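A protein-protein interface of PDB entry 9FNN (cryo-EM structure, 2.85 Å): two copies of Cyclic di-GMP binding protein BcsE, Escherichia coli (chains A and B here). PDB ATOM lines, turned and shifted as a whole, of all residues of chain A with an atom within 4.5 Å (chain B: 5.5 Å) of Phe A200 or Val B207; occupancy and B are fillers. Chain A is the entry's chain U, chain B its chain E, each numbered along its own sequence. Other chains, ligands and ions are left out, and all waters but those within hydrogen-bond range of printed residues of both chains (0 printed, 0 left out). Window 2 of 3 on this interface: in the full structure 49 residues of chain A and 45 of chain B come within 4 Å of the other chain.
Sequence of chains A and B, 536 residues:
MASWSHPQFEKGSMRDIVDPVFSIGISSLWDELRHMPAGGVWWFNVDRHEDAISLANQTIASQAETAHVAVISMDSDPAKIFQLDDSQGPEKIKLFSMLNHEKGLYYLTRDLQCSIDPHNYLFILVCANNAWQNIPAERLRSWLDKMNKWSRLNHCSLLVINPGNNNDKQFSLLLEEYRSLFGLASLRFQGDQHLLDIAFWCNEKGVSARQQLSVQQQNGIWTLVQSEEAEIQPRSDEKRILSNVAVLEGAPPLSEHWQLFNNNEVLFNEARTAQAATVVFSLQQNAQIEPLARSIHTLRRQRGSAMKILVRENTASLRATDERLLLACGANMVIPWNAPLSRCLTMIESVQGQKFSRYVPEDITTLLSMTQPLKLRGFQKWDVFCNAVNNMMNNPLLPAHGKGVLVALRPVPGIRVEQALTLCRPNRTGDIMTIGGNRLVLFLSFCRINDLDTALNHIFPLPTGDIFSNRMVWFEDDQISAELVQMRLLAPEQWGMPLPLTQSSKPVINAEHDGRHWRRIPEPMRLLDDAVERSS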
ATOM      1  N   LEU A 174       7.491  15.532  10.560  1.00  0.00           N
ATOM      2  CA  LEU A 174       6.230  16.259  10.483  1.00  0.00           C
ATOM      3  C   LEU A 174       5.600  16.148   9.101  1.00  0.00           C
ATOM      4  O   LEU A 174       4.368  16.146   8.982  1.00  0.00           O
ATOM      5  CB  LEU A 174       6.451  17.721  10.862  1.00  0.00           C
ATOM      6  CG  LEU A 174       6.951  17.954  12.289  1.00  0.00           C
ATOM      7  CD1 LEU A 174       7.558  19.335  12.418  1.00  0.00           C
ATOM      8  CD2 LEU A 174       5.833  17.771  13.299  1.00  0.00           C
ATOM      9  N   LEU A 175       6.417  16.062   8.050  1.00  0.00           N
ATOM     10  CA  LEU A 175       5.889  15.814   6.712  1.00  0.00           C
ATOM     11  C   LEU A 175       5.186  14.469   6.646  1.00  0.00           C
ATOM     12  O   LEU A 175       4.096  14.353   6.075  1.00  0.00           O
ATOM     13  CB  LEU A 175       7.012  15.869   5.678  1.00  0.00           C
ATOM     14  CG  LEU A 175       7.578  17.236   5.302  1.00  0.00           C
ATOM     15  CD1 LEU A 175       8.715  17.080   4.304  1.00  0.00           C
ATOM     16  CD2 LEU A 175       6.482  18.109   4.732  1.00  0.00           C
ATOM     17  N   TYR A 178       1.058  13.519   8.455  1.00  0.00           N
ATOM     18  CA  TYR A 178      -0.137  14.197   7.965  1.00  0.00           C
ATOM     19  C   TYR A 178      -1.337  13.917   8.857  1.00  0.00           C
ATOM     20  O   TYR A 178      -2.138  14.817   9.130  1.00  0.00           O
ATOM     21  CB  TYR A 178      -0.448  13.785   6.528  1.00  0.00           C
ATOM     22  CG  TYR A 178      -1.813  14.262   6.077  1.00  0.00           C
ATOM     23  CD1 TYR A 178      -2.005  15.565   5.642  1.00  0.00           C
ATOM     24  CD2 TYR A 178      -2.913  13.415   6.103  1.00  0.00           C
ATOM     25  CE1 TYR A 178      -3.251  16.007   5.240  1.00  0.00           C
ATOM     26  CE2 TYR A 178      -4.161  13.849   5.705  1.00  0.00           C
ATOM     27  CZ  TYR A 178      -4.325  15.144   5.274  1.00  0.00           C
ATOM     28  OH  TYR A 178      -5.568  15.574   4.875  1.00  0.00           O
ATOM     29  N   LEU A 181      -1.611  16.293  11.754  1.00  0.00           N
ATOM     30  CA  LEU A 181      -1.393  17.712  11.498  1.00  0.00           C
ATOM     31  C   LEU A 181      -2.254  18.147  10.324  1.00  0.00           C
ATOM     32  O   LEU A 181      -2.137  17.591   9.227  1.00  0.00           O
ATOM     33  CB  LEU A 181       0.082  17.995  11.204  1.00  0.00           C
ATOM     34  CG  LEU A 181       1.057  17.750  12.349  1.00  0.00           C
ATOM     35  CD1 LEU A 181       2.477  18.003  11.888  1.00  0.00           C
ATOM     36  CD2 LEU A 181       0.704  18.639  13.523  1.00  0.00           C
ATOM     37  N   PHE A 182      -3.112  19.140  10.552  1.00  0.00           N
ATOM     38  CA  PHE A 182      -3.859  19.727   9.446  1.00  0.00           C
ATOM     39  C   PHE A 182      -2.928  20.421   8.458  1.00  0.00           C
ATOM     40  O   PHE A 182      -3.080  20.265   7.241  1.00  0.00           O
ATOM     41  CB  PHE A 182      -4.893  20.716   9.972  1.00  0.00           C
ATOM     42  CG  PHE A 182      -6.183  20.089  10.394  1.00  0.00           C
ATOM     43  CD1 PHE A 182      -6.198  18.946  11.163  1.00  0.00           C
ATOM     44  CD2 PHE A 182      -7.385  20.670  10.047  1.00  0.00           C
ATOM     45  CE1 PHE A 182      -7.388  18.388  11.558  1.00  0.00           C
ATOM     46  CE2 PHE A 182      -8.574  20.118  10.437  1.00  0.00           C
ATOM     47  CZ  PHE A 182      -8.579  18.979  11.193  1.00  0.00           C
ATOM     48  N   GLY A 183      -1.959  21.184   8.958  1.00  0.00           N
ATOM     49  CA  GLY A 183      -1.073  21.930   8.087  1.00  0.00           C
ATOM     50  C   GLY A 183       0.293  22.220   8.670  1.00  0.00           C
ATOM     51  O   GLY A 183       0.409  22.669   9.813  1.00  0.00           O
ATOM     52  N   LEU A 184       1.336  21.971   7.885  1.00  0.00           N
ATOM     53  CA  LEU A 184       2.717  22.216   8.280  1.00  0.00           C
ATOM     54  C   LEU A 184       3.253  23.406   7.495  1.00  0.00           C
ATOM     55  O   LEU A 184       3.334  23.354   6.262  1.00  0.00           O
ATOM     56  CB  LEU A 184       3.580  20.981   8.033  1.00  0.00           C
ATOM     57  CG  LEU A 184       5.065  21.125   8.358  1.00  0.00           C
ATOM     58  CD1 LEU A 184       5.255  21.393   9.838  1.00  0.00           C
ATOM     59  CD2 LEU A 184       5.829  19.884   7.929  1.00  0.00           C
ATOM     60  N   ILE A 198       4.834  26.574   2.820  1.00  0.00           N
ATOM     61  CA  ILE A 198       3.780  25.724   3.357  1.00  0.00           C
ATOM     62  C   ILE A 198       3.782  24.430   2.554  1.00  0.00           C
ATOM     63  O   ILE A 198       3.410  24.419   1.375  1.00  0.00           O
ATOM     64  CB  ILE A 198       2.411  26.410   3.300  1.00  0.00           C
ATOM     65  CG1 ILE A 198       2.488  27.811   3.900  1.00  0.00           C
ATOM     66  CG2 ILE A 198       1.371  25.577   4.030  1.00  0.00           C
ATOM     67  CD1 ILE A 198       2.275  28.909   2.881  1.00  0.00           C
ATOM     68  N   ALA A 199       4.218  23.338   3.188  1.00  0.00           N
ATOM     69  CA  ALA A 199       4.196  22.038   2.528  1.00  0.00           C
ATOM     70  C   ALA A 199       2.766  21.584   2.261  1.00  0.00           C
ATOM     71  O   ALA A 199       2.451  21.102   1.167  1.00  0.00           O
ATOM     72  CB  ALA A 199       4.941  21.009   3.375  1.00  0.00           C
ATOM     73  N   PHE A 200       1.889  21.724   3.253  1.00  0.00           N
ATOM     74  CA  PHE A 200       0.463  21.514   3.048  1.00  0.00           C
ATOM     75  C   PHE A 200      -0.299  22.287   4.111  1.00  0.00           C
ATOM     76  O   PHE A 200       0.234  22.602   5.178  1.00  0.00           O
ATOM     77  CB  PHE A 200       0.087  20.023   3.065  1.00  0.00           C
ATOM     78  CG  PHE A 200       0.441  19.308   4.339  1.00  0.00           C
ATOM     79  CD1 PHE A 200      -0.415  19.331   5.428  1.00  0.00           C
ATOM     80  CD2 PHE A 200       1.618  18.591   4.438  1.00  0.00           C
ATOM     81  CE1 PHE A 200      -0.092  18.673   6.593  1.00  0.00           C
ATOM     82  CE2 PHE A 200       1.944  17.929   5.603  1.00  0.00           C
ATOM     83  CZ  PHE A 200       1.087  17.970   6.680  1.00  0.00           C
ATOM     84  N   TRP A 201      -1.554  22.596   3.800  1.00  0.00           N
ATOM     85  CA  TRP A 201      -2.420  23.336   4.704  1.00  0.00           C
ATOM     86  C   TRP A 201      -3.863  23.015   4.356  1.00  0.00           C
ATOM     87  O   TRP A 201      -4.211  22.903   3.180  1.00  0.00           O
ATOM     88  CB  TRP A 201      -2.174  24.844   4.613  1.00  0.00           C
ATOM     89  CG  TRP A 201      -2.907  25.638   5.647  1.00  0.00           C
ATOM     90  CD1 TRP A 201      -4.224  25.990   5.631  1.00  0.00           C
ATOM     91  CD2 TRP A 201      -2.361  26.185   6.850  1.00  0.00           C
ATOM     92  NE1 TRP A 201      -4.533  26.719   6.750  1.00  0.00           N
ATOM     93  CE2 TRP A 201      -3.406  26.852   7.516  1.00  0.00           C
ATOM     94  CE3 TRP A 201      -1.091  26.175   7.428  1.00  0.00           C
ATOM     95  CZ2 TRP A 201      -3.219  27.499   8.728  1.00  0.00           C
ATOM     96  CZ3 TRP A 201      -0.909  26.815   8.628  1.00  0.00           C
ATOM     97  CH2 TRP A 201      -1.967  27.470   9.268  1.00  0.00           C
ATOM     98  N   SER A 208      -4.396  22.942   0.455  1.00  0.00           N
ATOM     99  CA  SER A 208      -3.337  23.518  -0.358  1.00  0.00           C
ATOM    100  C   SER A 208      -2.024  22.841  -0.005  1.00  0.00           C
ATOM    101  O   SER A 208      -1.751  22.583   1.169  1.00  0.00           O
ATOM    102  CB  SER A 208      -3.224  25.027  -0.134  1.00  0.00           C
ATOM    103  OG  SER A 208      -2.957  25.320   1.226  1.00  0.00           O
ATOM    104  N   ALA A 209      -1.212  22.550  -1.018  1.00  0.00           N
ATOM    105  CA  ALA A 209       0.002  21.776  -0.813  1.00  0.00           C
ATOM    106  C   ALA A 209       1.139  22.318  -1.664  1.00  0.00           C
ATOM    107  O   ALA A 209       0.955  22.623  -2.845  1.00  0.00           O
ATOM    108  CB  ALA A 209      -0.223  20.294  -1.135  1.00  0.00           C
ATOM    109  N   ARG A 210       2.320  22.417  -1.048  1.00  0.00           N
ATOM    110  CA  ARG A 210       3.553  22.852  -1.704  1.00  0.00           C
ATOM    111  C   ARG A 210       3.417  24.264  -2.278  1.00  0.00           C
ATOM    112  O   ARG A 210       3.504  24.489  -3.487  1.00  0.00           O
ATOM    113  CB  ARG A 210       3.979  21.853  -2.786  1.00  0.00           C
ATOM    114  CG  ARG A 210       5.485  21.657  -2.870  1.00  0.00           C
ATOM    115  CD  ARG A 210       6.033  21.103  -1.562  1.00  0.00           C
ATOM    116  NE  ARG A 210       7.486  20.968  -1.582  1.00  0.00           N
ATOM    117  CZ  ARG A 210       8.329  21.875  -1.105  1.00  0.00           C
ATOM    118  NH1 ARG A 210       7.899  23.002  -0.563  1.00  0.00           N
ATOM    119  NH2 ARG A 210       9.637  21.641  -1.172  1.00  0.00           N
ATOM    120  N   TRP B 201      -3.811  14.060  -2.364  1.00  0.00           N
ATOM    121  CA  TRP B 201      -3.191  12.770  -2.110  1.00  0.00           C
ATOM    122  C   TRP B 201      -2.230  12.920  -0.945  1.00  0.00           C
ATOM    123  O   TRP B 201      -1.469  13.889  -0.883  1.00  0.00           O
ATOM    124  CB  TRP B 201      -2.451  12.250  -3.344  1.00  0.00           C
ATOM    125  CG  TRP B 201      -2.493  10.767  -3.483  1.00  0.00           C
ATOM    126  CD1 TRP B 201      -1.560   9.877  -3.050  1.00  0.00           C
ATOM    127  CD2 TRP B 201      -3.528   9.995  -4.101  1.00  0.00           C
ATOM    128  NE1 TRP B 201      -1.947   8.599  -3.359  1.00  0.00           N
ATOM    129  CE2 TRP B 201      -3.154   8.644  -4.004  1.00  0.00           C
ATOM    130  CE3 TRP B 201      -4.737  10.316  -4.726  1.00  0.00           C
ATOM    131  CZ2 TRP B 201      -3.942   7.615  -4.509  1.00  0.00           C
ATOM    132  CZ3 TRP B 201      -5.516   9.291  -5.226  1.00  0.00           C
ATOM    133  CH2 TRP B 201      -5.116   7.960  -5.114  1.00  0.00           C
ATOM    134  N   CYS B 202      -2.269  11.961  -0.026  1.00  0.00           N
ATOM    135  CA  CYS B 202      -1.424  11.976   1.162  1.00  0.00           C
ATOM    136  C   CYS B 202      -0.735  10.626   1.273  1.00  0.00           C
ATOM    137  O   CYS B 202      -1.389   9.611   1.533  1.00  0.00           O
ATOM    138  CB  CYS B 202      -2.242  12.277   2.416  1.00  0.00           C
ATOM    139  SG  CYS B 202      -3.198  13.804   2.320  1.00  0.00           S
ATOM    140  N   ASN B 203       0.580  10.611   1.080  1.00  0.00           N
ATOM    141  CA  ASN B 203       1.350   9.379   1.128  1.00  0.00           C
ATOM    142  C   ASN B 203       2.653   9.655   1.868  1.00  0.00           C
ATOM    143  O   ASN B 203       2.814  10.692   2.519  1.00  0.00           O
ATOM    144  CB  ASN B 203       1.583   8.823  -0.281  1.00  0.00           C
ATOM    145  CG  ASN B 203       2.283   9.805  -1.189  1.00  0.00           C
ATOM    146  OD1 ASN B 203       1.968  10.993  -1.198  1.00  0.00           O
ATOM    147  ND2 ASN B 203       3.243   9.313  -1.963  1.00  0.00           N
ATOM    148  N   LYS B 205       5.669  10.220   0.743  1.00  0.00           N
ATOM    149  CA  LYS B 205       6.594  11.157   0.122  1.00  0.00           C
ATOM    150  C   LYS B 205       6.067  12.584   0.058  1.00  0.00           C
ATOM    151  O   LYS B 205       6.742  13.449  -0.510  1.00  0.00           O
ATOM    152  CB  LYS B 205       6.957  10.679  -1.287  1.00  0.00           C
ATOM    153  CG  LYS B 205       7.704   9.358  -1.318  1.00  0.00           C
ATOM    154  CD  LYS B 205       8.058   8.951  -2.739  1.00  0.00           C
ATOM    155  CE  LYS B 205       8.831   7.645  -2.755  1.00  0.00           C
ATOM    156  NZ  LYS B 205       9.204   7.226  -4.133  1.00  0.00           N
ATOM    157  N   GLY B 206       4.892  12.860   0.612  1.00  0.00           N
ATOM    158  CA  GLY B 206       4.388  14.212   0.677  1.00  0.00           C
ATOM    159  C   GLY B 206       2.902  14.267   0.389  1.00  0.00           C
ATOM    160  O   GLY B 206       2.212  13.251   0.362  1.00  0.00           O
ATOM    161  N   VAL B 207       2.413  15.487   0.178  1.00  0.00           N
ATOM    162  CA  VAL B 207       1.001  15.757  -0.062  1.00  0.00           C
ATOM    163  C   VAL B 207       0.872  16.583  -1.334  1.00  0.00           C
ATOM    164  O   VAL B 207       1.632  17.534  -1.547  1.00  0.00           O
ATOM    165  CB  VAL B 207       0.351  16.490   1.131  1.00  0.00           C
ATOM    166  CG1 VAL B 207      -1.113  16.767   0.857  1.00  0.00           C
ATOM    167  CG2 VAL B 207       0.509  15.677   2.400  1.00  0.00           C
ATOM    168  N   SER B 208      -0.087  16.218  -2.177  1.00  0.00           N
ATOM    169  CA  SER B 208      -0.358  16.914  -3.425  1.00  0.00           C
ATOM    170  C   SER B 208      -1.692  17.641  -3.329  1.00  0.00           C
ATOM    171  O   SER B 208      -2.476  17.421  -2.405  1.00  0.00           O
ATOM    172  CB  SER B 208      -0.374  15.940  -4.606  1.00  0.00           C
ATOM    173  OG  SER B 208       0.836  15.210  -4.683  1.00  0.00           O
ATOM    174  N   ALA B 209      -1.933  18.532  -4.288  1.00  0.00           N
ATOM    175  CA  ALA B 209      -3.182  19.287  -4.315  1.00  0.00           C
ATOM    176  C   ALA B 209      -3.501  19.722  -5.736  1.00  0.00           C
ATOM    177  O   ALA B 209      -2.762  20.517  -6.322  1.00  0.00           O
ATOM    178  CB  ALA B 209      -3.104  20.500  -3.392  1.00  0.00           C
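The backbone NH (N) of Ser B208 lies within hydrogen-bond range of the backbone carbonyl oxygen (O) of Trp B201. N of Leu A184 sits at hydrogen-bond distance from O of Phe A200.
Ala A209 touches Ser B208, but with the chains exchanged Ser A208 does not touch Ala B209 (4.3 Å). Ala B209 touches its own counterpart, Ala A209.
Cys B202 touches Tyr A178. CD2 of Phe A200 touches CG2 of Val B207, 3.7 Å away. Ala A209 touches Val B207 (CB to O, 3.4 Å). Ser B208 touches Ala A209. Ala B209 touches Ala A209.
Printed residues of chain B that touch a printed residue of chain A: Cys B202, Val B207, Ser B208 and Ala B209. Printed residues of chain A that touch a printed residue of chain B: Tyr A178, Phe A200 and Ala A209. Hydrophobic or aromatic side chains of chain A within 4 Å of the printed part of chain B: Tyr A178, Phe A200 and Ala A209. Among the printed residues, 5 pairs touch across the chains. Among the printed residues, no Asp or Glu carboxylate lies within 4 Å of a Lys or Arg side-chain nitrogen of the other chain.
Phe A200 touches one residue of chain B. Of the printed residues of chain A, Val B207 touches Phe A200 and Ala A209. Of the printed residues of chain A, Ser B208 touches Ala A209. Printed residues of chain A within 4 Å of Cys B202: Tyr A178 (3.4 Å). The nearest printed residue of chain B that does not touch Phe A200 is Gly B206 (6.1 Å).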
